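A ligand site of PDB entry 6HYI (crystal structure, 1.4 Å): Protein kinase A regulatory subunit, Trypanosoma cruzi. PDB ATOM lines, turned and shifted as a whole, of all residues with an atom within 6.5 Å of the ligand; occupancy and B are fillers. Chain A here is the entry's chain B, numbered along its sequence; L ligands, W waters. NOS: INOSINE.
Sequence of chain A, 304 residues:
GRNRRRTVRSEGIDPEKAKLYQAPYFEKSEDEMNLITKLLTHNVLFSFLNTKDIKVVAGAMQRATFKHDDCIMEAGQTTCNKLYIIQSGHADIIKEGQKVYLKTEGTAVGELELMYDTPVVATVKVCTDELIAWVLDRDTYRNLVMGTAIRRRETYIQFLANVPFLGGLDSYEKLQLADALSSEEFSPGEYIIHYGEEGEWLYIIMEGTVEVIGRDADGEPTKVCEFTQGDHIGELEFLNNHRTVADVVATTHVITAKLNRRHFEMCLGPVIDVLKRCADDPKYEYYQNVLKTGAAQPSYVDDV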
ATOM      1  N   MET A  73      27.970 -13.094   0.554  1.00  0.00           N
ATOM      2  CA  MET A  73      26.568 -13.080   0.932  1.00  0.00           C
ATOM      3  C   MET A  73      26.447 -12.204   2.161  1.00  0.00           C
ATOM      4  O   MET A  73      27.423 -11.952   2.872  1.00  0.00           O
ATOM      5  CB  MET A  73      26.046 -14.507   1.194  1.00  0.00           C
ATOM      6  CG  MET A  73      26.876 -15.278   2.210  1.00  0.00           C
ATOM      7  SD  MET A  73      26.479 -17.038   2.259  1.00  0.00           S
ATOM      8  CE  MET A  73      27.304 -17.596   0.771  1.00  0.00           C
ATOM      9  N   ILE A  93      33.639 -14.229   8.575  1.00  0.00           N
ATOM     10  CA  ILE A  93      32.238 -14.414   8.929  1.00  0.00           C
ATOM     11  C   ILE A  93      31.890 -13.338   9.952  1.00  0.00           C
ATOM     12  O   ILE A  93      32.533 -13.242  10.997  1.00  0.00           O
ATOM     13  CB  ILE A  93      32.003 -15.820   9.505  1.00  0.00           C
ATOM     14  CG1 ILE A  93      32.477 -16.903   8.517  1.00  0.00           C
ATOM     15  CG2 ILE A  93      30.529 -15.999   9.869  1.00  0.00           C
ATOM     16  CD1 ILE A  93      31.792 -16.831   7.161  1.00  0.00           C
ATOM     17  N   LYS A  95      28.941 -11.417  12.275  1.00  0.00           N
ATOM     18  CA  LYS A  95      27.632 -11.393  12.912  1.00  0.00           C
ATOM     19  C   LYS A  95      27.534 -10.123  13.749  1.00  0.00           C
ATOM     20  O   LYS A  95      28.371  -9.896  14.631  1.00  0.00           O
ATOM     21  CB  LYS A  95      27.457 -12.600  13.839  1.00  0.00           C
ATOM     22  CG  LYS A  95      27.552 -13.951  13.143  1.00  0.00           C
ATOM     23  CD  LYS A  95      27.174 -15.071  14.092  1.00  0.00           C
ATOM     24  CE  LYS A  95      27.376 -16.430  13.439  1.00  0.00           C
ATOM     25  NZ  LYS A  95      27.181 -17.522  14.418  1.00  0.00           N
ATOM     26  N   VAL A 100      33.664 -13.198  13.576  1.00  0.00           N
ATOM     27  CA  VAL A 100      33.542 -14.342  14.480  1.00  0.00           C
ATOM     28  C   VAL A 100      34.220 -15.608  13.962  1.00  0.00           C
ATOM     29  O   VAL A 100      34.336 -16.583  14.722  1.00  0.00           O
ATOM     30  CB  VAL A 100      32.069 -14.630  14.851  1.00  0.00           C
ATOM     31  CG1 VAL A 100      31.446 -13.417  15.517  1.00  0.00           C
ATOM     32  CG2 VAL A 100      31.278 -15.039  13.612  1.00  0.00           C
ATOM     33  N   TYR A 101      34.678 -15.632  12.713  1.00  0.00           N
ATOM     34  CA  TYR A 101      35.255 -16.848  12.150  1.00  0.00           C
ATOM     35  C   TYR A 101      35.977 -16.457  10.869  1.00  0.00           C
ATOM     36  O   TYR A 101      35.578 -15.498  10.206  1.00  0.00           O
ATOM     37  CB  TYR A 101      34.162 -17.855  11.828  1.00  0.00           C
ATOM     38  CG  TYR A 101      34.653 -19.254  11.568  1.00  0.00           C
ATOM     39  CD1 TYR A 101      34.895 -20.130  12.619  1.00  0.00           C
ATOM     40  CD2 TYR A 101      34.868 -19.706  10.272  1.00  0.00           C
ATOM     41  CE1 TYR A 101      35.337 -21.416  12.378  1.00  0.00           C
ATOM     42  CE2 TYR A 101      35.314 -20.984  10.029  1.00  0.00           C
ATOM     43  CZ  TYR A 101      35.544 -21.840  11.089  1.00  0.00           C
ATOM     44  OH  TYR A 101      35.992 -23.109  10.842  1.00  0.00           O
ATOM     45  N   LEU A 102      37.023 -17.196  10.537  1.00  0.00           N
ATOM     46  CA  LEU A 102      37.797 -16.955   9.322  1.00  0.00           C
ATOM     47  C   LEU A 102      37.723 -18.180   8.421  1.00  0.00           C
ATOM     48  O   LEU A 102      38.129 -19.276   8.814  1.00  0.00           O
ATOM     49  CB  LEU A 102      39.255 -16.622   9.659  1.00  0.00           C
ATOM     50  CG  LEU A 102      40.173 -16.309   8.465  1.00  0.00           C
ATOM     51  CD1 LEU A 102      39.826 -14.963   7.867  1.00  0.00           C
ATOM     52  CD2 LEU A 102      41.638 -16.367   8.869  1.00  0.00           C
ATOM     53  N   LYS A 103      37.185 -17.991   7.213  1.00  0.00           N
ATOM     54  CA  LYS A 103      37.126 -19.048   6.209  1.00  0.00           C
ATOM     55  C   LYS A 103      38.352 -18.949   5.317  1.00  0.00           C
ATOM     56  O   LYS A 103      38.667 -17.867   4.811  1.00  0.00           O
ATOM     57  CB  LYS A 103      35.868 -18.891   5.353  1.00  0.00           C
ATOM     58  CG  LYS A 103      34.564 -19.250   6.078  1.00  0.00           C
ATOM     59  CD  LYS A 103      34.335 -20.735   6.174  1.00  0.00           C
ATOM     60  CE  LYS A 103      32.991 -21.055   6.848  1.00  0.00           C
ATOM     61  NZ  LYS A 103      32.711 -22.506   6.843  1.00  0.00           N
ATOM     62  N   ALA A 108      33.967 -24.055   2.829  1.00  0.00           N
ATOM     63  CA  ALA A 108      32.717 -23.715   2.172  1.00  0.00           C
ATOM     64  C   ALA A 108      32.010 -22.581   2.907  1.00  0.00           C
ATOM     65  O   ALA A 108      32.125 -22.437   4.122  1.00  0.00           O
ATOM     66  CB  ALA A 108      31.797 -24.932   2.130  1.00  0.00           C
ATOM     67  N   VAL A 109      31.277 -21.786   2.135  1.00  0.00           N
ATOM     68  CA  VAL A 109      30.306 -20.859   2.708  1.00  0.00           C
ATOM     69  C   VAL A 109      28.971 -21.047   2.000  1.00  0.00           C
ATOM     70  O   VAL A 109      28.920 -21.339   0.803  1.00  0.00           O
ATOM     71  CB  VAL A 109      30.743 -19.385   2.677  1.00  0.00           C
ATOM     72  CG1 VAL A 109      31.927 -19.169   3.600  1.00  0.00           C
ATOM     73  CG2 VAL A 109      31.051 -18.956   1.250  1.00  0.00           C
ATOM     74  N   GLY A 110      27.894 -20.845   2.753  1.00  0.00           N
ATOM     75  CA  GLY A 110      26.561 -21.018   2.236  1.00  0.00           C
ATOM     76  C   GLY A 110      25.928 -22.345   2.606  1.00  0.00           C
ATOM     77  O   GLY A 110      24.750 -22.556   2.309  1.00  0.00           O
ATOM     78  N   GLU A 111      26.698 -23.242   3.230  1.00  0.00           N
ATOM     79  CA  GLU A 111      26.184 -24.576   3.509  1.00  0.00           C
ATOM     80  C   GLU A 111      25.145 -24.579   4.618  1.00  0.00           C
ATOM     81  O   GLU A 111      24.234 -25.417   4.615  1.00  0.00           O
ATOM     82  CB  GLU A 111      27.343 -25.523   3.835  1.00  0.00           C
ATOM     83  CG  GLU A 111      27.799 -25.535   5.294  1.00  0.00           C
ATOM     84  CD  GLU A 111      28.451 -24.242   5.782  1.00  0.00           C
ATOM     85  OE1 GLU A 111      28.572 -24.092   7.016  1.00  0.00           O
ATOM     86  OE2 GLU A 111      28.836 -23.381   4.954  1.00  0.00           O
ATOM     87  N   LEU A 112      25.259 -23.659   5.576  1.00  0.00           N
ATOM     88  CA  LEU A 112      24.273 -23.592   6.649  1.00  0.00           C
ATOM     89  C   LEU A 112      22.888 -23.307   6.083  1.00  0.00           C
ATOM     90  O   LEU A 112      21.898 -23.964   6.437  1.00  0.00           O
ATOM     91  CB  LEU A 112      24.700 -22.525   7.650  1.00  0.00           C
ATOM     92  CG  LEU A 112      23.988 -22.331   8.981  1.00  0.00           C
ATOM     93  CD1 LEU A 112      24.823 -21.413   9.855  1.00  0.00           C
ATOM     94  CD2 LEU A 112      22.605 -21.754   8.782  1.00  0.00           C
ATOM     95  N   GLU A 113      22.805 -22.350   5.155  1.00  0.00           N
ATOM     96  CA  GLU A 113      21.525 -21.962   4.571  1.00  0.00           C
ATOM     97  C   GLU A 113      20.953 -23.076   3.705  1.00  0.00           C
ATOM     98  O   GLU A 113      19.739 -23.275   3.676  1.00  0.00           O
ATOM     99  CB  GLU A 113      21.727 -20.710   3.731  1.00  0.00           C
ATOM    100  CG  GLU A 113      22.057 -19.488   4.550  1.00  0.00           C
ATOM    101  CD  GLU A 113      23.445 -19.481   5.180  1.00  0.00           C
ATOM    102  OE1 GLU A 113      24.376 -20.161   4.664  1.00  0.00           O
ATOM    103  OE2 GLU A 113      23.608 -18.761   6.184  1.00  0.00           O
ATOM    104  N   LEU A 114      21.812 -23.790   2.972  1.00  0.00           N
ATOM    105  CA  LEU A 114      21.337 -24.858   2.107  1.00  0.00           C
ATOM    106  C   LEU A 114      20.911 -26.072   2.911  1.00  0.00           C
ATOM    107  O   LEU A 114      19.937 -26.749   2.561  1.00  0.00           O
ATOM    108  CB  LEU A 114      22.429 -25.230   1.089  1.00  0.00           C
ATOM    109  CG  LEU A 114      22.618 -24.253  -0.053  1.00  0.00           C
ATOM    110  CD1 LEU A 114      23.900 -24.563  -0.823  1.00  0.00           C
ATOM    111  CD2 LEU A 114      21.427 -24.316  -0.992  1.00  0.00           C
ATOM    112  N   PRO A 119      17.330 -18.030   5.568  1.00  0.00           N
ATOM    113  CA  PRO A 119      18.046 -16.916   4.967  1.00  0.00           C
ATOM    114  C   PRO A 119      19.454 -16.827   5.536  1.00  0.00           C
ATOM    115  O   PRO A 119      19.749 -17.350   6.617  1.00  0.00           O
ATOM    116  CB  PRO A 119      17.215 -15.682   5.348  1.00  0.00           C
ATOM    117  CG  PRO A 119      16.352 -16.125   6.482  1.00  0.00           C
ATOM    118  CD  PRO A 119      16.110 -17.593   6.285  1.00  0.00           C
ATOM    119  N   VAL A 120      20.334 -16.152   4.800  1.00  0.00           N
ATOM    120  CA  VAL A 120      21.727 -16.058   5.189  1.00  0.00           C
ATOM    121  C   VAL A 120      21.843 -15.605   6.636  1.00  0.00           C
ATOM    122  O   VAL A 120      21.218 -14.608   7.045  1.00  0.00           O
ATOM    123  CB  VAL A 120      22.498 -15.111   4.245  1.00  0.00           C
ATOM    124  CG1 VAL A 120      23.911 -14.900   4.758  1.00  0.00           C
ATOM    125  CG2 VAL A 120      22.502 -15.668   2.839  1.00  0.00           C
ATOM    126  N   VAL A 121      22.624 -16.338   7.409  1.00  0.00           N
ATOM    127  CA  VAL A 121      22.753 -16.085   8.840  1.00  0.00           C
ATOM    128  C   VAL A 121      23.829 -15.057   9.141  1.00  0.00           C
ATOM    129  O   VAL A 121      23.651 -14.221  10.031  1.00  0.00           O
ATOM    130  CB  VAL A 121      23.006 -17.406   9.570  1.00  0.00           C
ATOM    131  CG1 VAL A 121      23.485 -17.129  10.989  1.00  0.00           C
ATOM    132  CG2 VAL A 121      21.762 -18.272   9.553  1.00  0.00           C
ATOM    133  N   ALA A 122      24.944 -15.110   8.433  1.00  0.00           N
ATOM    134  CA  ALA A 122      26.081 -14.238   8.701  1.00  0.00           C
ATOM    135  C   ALA A 122      26.587 -13.654   7.385  1.00  0.00           C
ATOM    136  O   ALA A 122      26.466 -14.273   6.330  1.00  0.00           O
ATOM    137  CB  ALA A 122      27.230 -15.004   9.351  1.00  0.00           C
ATOM    138  N   THR A 123      27.134 -12.454   7.467  1.00  0.00           N
ATOM    139  CA  THR A 123      27.795 -11.850   6.312  1.00  0.00           C
ATOM    140  C   THR A 123      29.154 -12.506   6.095  1.00  0.00           C
ATOM    141  O   THR A 123      29.879 -12.798   7.041  1.00  0.00           O
ATOM    142  CB  THR A 123      27.936 -10.348   6.544  1.00  0.00           C
ATOM    143  OG1 THR A 123      26.628  -9.766   6.579  1.00  0.00           O
ATOM    144  CG2 THR A 123      28.741  -9.686   5.436  1.00  0.00           C
ATOM    145  N   VAL A 124      29.474 -12.753   4.842  1.00  0.00           N
ATOM    146  CA  VAL A 124      30.749 -13.358   4.444  1.00  0.00           C
ATOM    147  C   VAL A 124      31.477 -12.299   3.646  1.00  0.00           C
ATOM    148  O   VAL A 124      31.056 -11.957   2.534  1.00  0.00           O
ATOM    149  CB  VAL A 124      30.531 -14.616   3.598  1.00  0.00           C
ATOM    150  CG1 VAL A 124      31.839 -15.245   3.196  1.00  0.00           C
ATOM    151  CG2 VAL A 124      29.667 -15.635   4.353  1.00  0.00           C
ATOM    152  N   ASP A 170      33.578 -24.884  19.044  1.00  0.00           N
ATOM    153  CA  ASP A 170      32.195 -24.462  19.243  1.00  0.00           C
ATOM    154  C   ASP A 170      31.255 -25.435  18.547  1.00  0.00           C
ATOM    155  O   ASP A 170      31.672 -26.433  17.947  1.00  0.00           O
ATOM    156  CB  ASP A 170      31.978 -23.015  18.793  1.00  0.00           C
ATOM    157  CG  ASP A 170      32.284 -22.804  17.316  1.00  0.00           C
ATOM    158  OD1 ASP A 170      32.204 -23.761  16.531  1.00  0.00           O
ATOM    159  OD2 ASP A 170      32.611 -21.655  16.940  1.00  0.00           O
ATOM    160  N   TYR A 172      29.429 -25.020  15.858  1.00  0.00           N
ATOM    161  CA  TYR A 172      29.633 -25.044  14.410  1.00  0.00           C
ATOM    162  C   TYR A 172      30.783 -25.966  14.039  1.00  0.00           C
ATOM    163  O   TYR A 172      30.683 -26.752  13.096  1.00  0.00           O
ATOM    164  CB  TYR A 172      29.875 -23.628  13.895  1.00  0.00           C
ATOM    165  CG  TYR A 172      30.061 -23.564  12.397  1.00  0.00           C
ATOM    166  CD1 TYR A 172      31.316 -23.731  11.837  1.00  0.00           C
ATOM    167  CD2 TYR A 172      28.992 -23.300  11.549  1.00  0.00           C
ATOM    168  CE1 TYR A 172      31.505 -23.669  10.458  1.00  0.00           C
ATOM    169  CE2 TYR A 172      29.166 -23.227  10.183  1.00  0.00           C
ATOM    170  CZ  TYR A 172      30.421 -23.408   9.648  1.00  0.00           C
ATOM    171  OH  TYR A 172      30.580 -23.343   8.278  1.00  0.00           O
ATOM    172  N   GLU A 173      31.901 -25.858  14.762  1.00  0.00           N
ATOM    173  CA  GLU A 173      33.080 -26.671  14.471  1.00  0.00           C
ATOM    174  C   GLU A 173      32.839 -28.146  14.796  1.00  0.00           C
ATOM    175  O   GLU A 173      33.319 -29.039  14.083  1.00  0.00           O
ATOM    176  CB  GLU A 173      34.275 -26.135  15.242  1.00  0.00           C
ATOM    177  CG  GLU A 173      34.710 -24.749  14.758  1.00  0.00           C
ATOM    178  CD  GLU A 173      35.720 -24.103  15.690  1.00  0.00           C
ATOM    179  OE1 GLU A 173      35.540 -24.200  16.924  1.00  0.00           O
ATOM    180  OE2 GLU A 173      36.671 -23.482  15.174  1.00  0.00           O
HETATM  181  N9  NOS L   1      28.833 -19.300   9.207  1.00  0.00           N
HETATM  182  C4  NOS L   1      29.652 -19.685  10.049  1.00  0.00           C
HETATM  183  N3  NOS L   1      30.893 -20.123  10.041  1.00  0.00           N
HETATM  184  C2  NOS L   1      31.522 -20.415  11.203  1.00  0.00           C
HETATM  185  N1  NOS L   1      30.889 -20.277  12.392  1.00  0.00           N
HETATM  186  C6  NOS L   1      29.645 -19.837  12.433  1.00  0.00           C
HETATM  187  O6  NOS L   1      29.105 -19.700  13.495  1.00  0.00           O
HETATM  188  C5  NOS L   1      29.004 -19.520  11.269  1.00  0.00           C
HETATM  189  N7  NOS L   1      27.711 -19.025  10.932  1.00  0.00           N
HETATM  190  C8  NOS L   1      27.704 -18.943   9.579  1.00  0.00           C
HETATM  191  C5' NOS L   1      26.648 -17.527   5.942  1.00  0.00           C
HETATM  192  O5' NOS L   1      25.801 -17.584   7.079  1.00  0.00           O
HETATM  193  C4' NOS L   1      27.753 -18.563   6.038  1.00  0.00           C
HETATM  194  O4' NOS L   1      28.695 -18.197   7.087  1.00  0.00           O
HETATM  195  C1' NOS L   1      29.056 -19.345   7.780  1.00  0.00           C
HETATM  196  C2' NOS L   1      28.572 -20.546   7.028  1.00  0.00           C
HETATM  197  O2' NOS L   1      29.508 -20.899   6.013  1.00  0.00           O
HETATM  198  C3' NOS L   1      27.306 -19.974   6.413  1.00  0.00           C
HETATM  199  O3' NOS L   1      26.799 -20.703   5.317  1.00  0.00           O
HETATM  200  O   HOH W   1      27.191 -21.371  14.926  1.00  0.00           O
HETATM  201  O   HOH W   2      25.669 -19.397  13.007  1.00  0.00           O
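The backbone NH (N) of Gly 110 is in hydrogen-bond range of an oxygen (O3') of the ligand.
The side-chain carboxylate of Glu 113 sits at hydrogen-bond distance from an oxygen (O3') of the ligand (2.6 Å).
An oxygen (O5') of the ligand sits at hydrogen-bond distance from the backbone NH of Ala 122, at 2.9 Å.
N of Glu 111 is in hydrogen-bond range of O3' of the ligand, at 3.3 Å.
The backbone NH of Val 121 sits at hydrogen-bond distance from an oxygen (O5') of the ligand, 3.4 Å away.
OE2 of Glu 111 sits at hydrogen-bond distance from O2' of the ligand (2.8 Å).
The backbone NH of Leu 112 lies within hydrogen-bond range of an oxygen (O3') of the ligand (3.3 Å).
O5' of the ligand sits close to O of Ala 122, at 3.5 Å.
NZ of Lys 95 is in hydrogen-bond range of O6 of the ligand, at 3.0 Å.
Residues that only touch the ligand: Met 73 (3.7 Å), Ile 93 (3.4 Å), Tyr 101 (3.4 Å), Lys 103 (3.6 Å), Ala 108 (3.6 Å), Val 109 (3.4 Å), Val 120 (3.97 Å), Val 124 (3.9 Å) and Tyr 172 (3.3 Å).
Hydrophobic or aromatic side chains within 4 Å of the ligand: Met 73, Ile 93, Tyr 101, Val 109, Leu 112, Val 120, Val 121, Ala 122, Val 124 and Tyr 172.
Within 4 Å of the ligand: Met 73, Ile 93, Lys 95, Tyr 101, Lys 103, Ala 108, Val 109, Gly 110, Glu 111, Leu 112, Glu 113, Val 120, Val 121, Ala 122, Val 124 and Tyr 172.
Water W2 lies within hydrogen-bond range of NZ of Lys 95 and N7 of the ligand.
O of Met 73 is in hydrogen-bond range of N of Val 124, 3.0 Å away.
The backbone carbonyl oxygen of Ala 108 is in hydrogen-bond range of the side-chain amino group of Lys 103, 2.8 Å away.
The side-chain hydroxyl (OH) of Tyr 172 lies within hydrogen-bond range of the side-chain amino group (NZ) of Lys 103, at 2.7 Å.
O of Tyr 101 lies within hydrogen-bond range of N of Ile 93 (2.8 Å).
O of Ile 93 sits at hydrogen-bond distance from N of Val 100.
OE1 of Glu 111 is in hydrogen-bond range of OH of Tyr 172.
N of Tyr 172 sits at hydrogen-bond distance from OD1 of Asp 170 (3.1 Å).
The backbone NH (N) of Val 121 lies within hydrogen-bond range of the side-chain carboxylate (OE2) of Glu 113 (2.9 Å).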
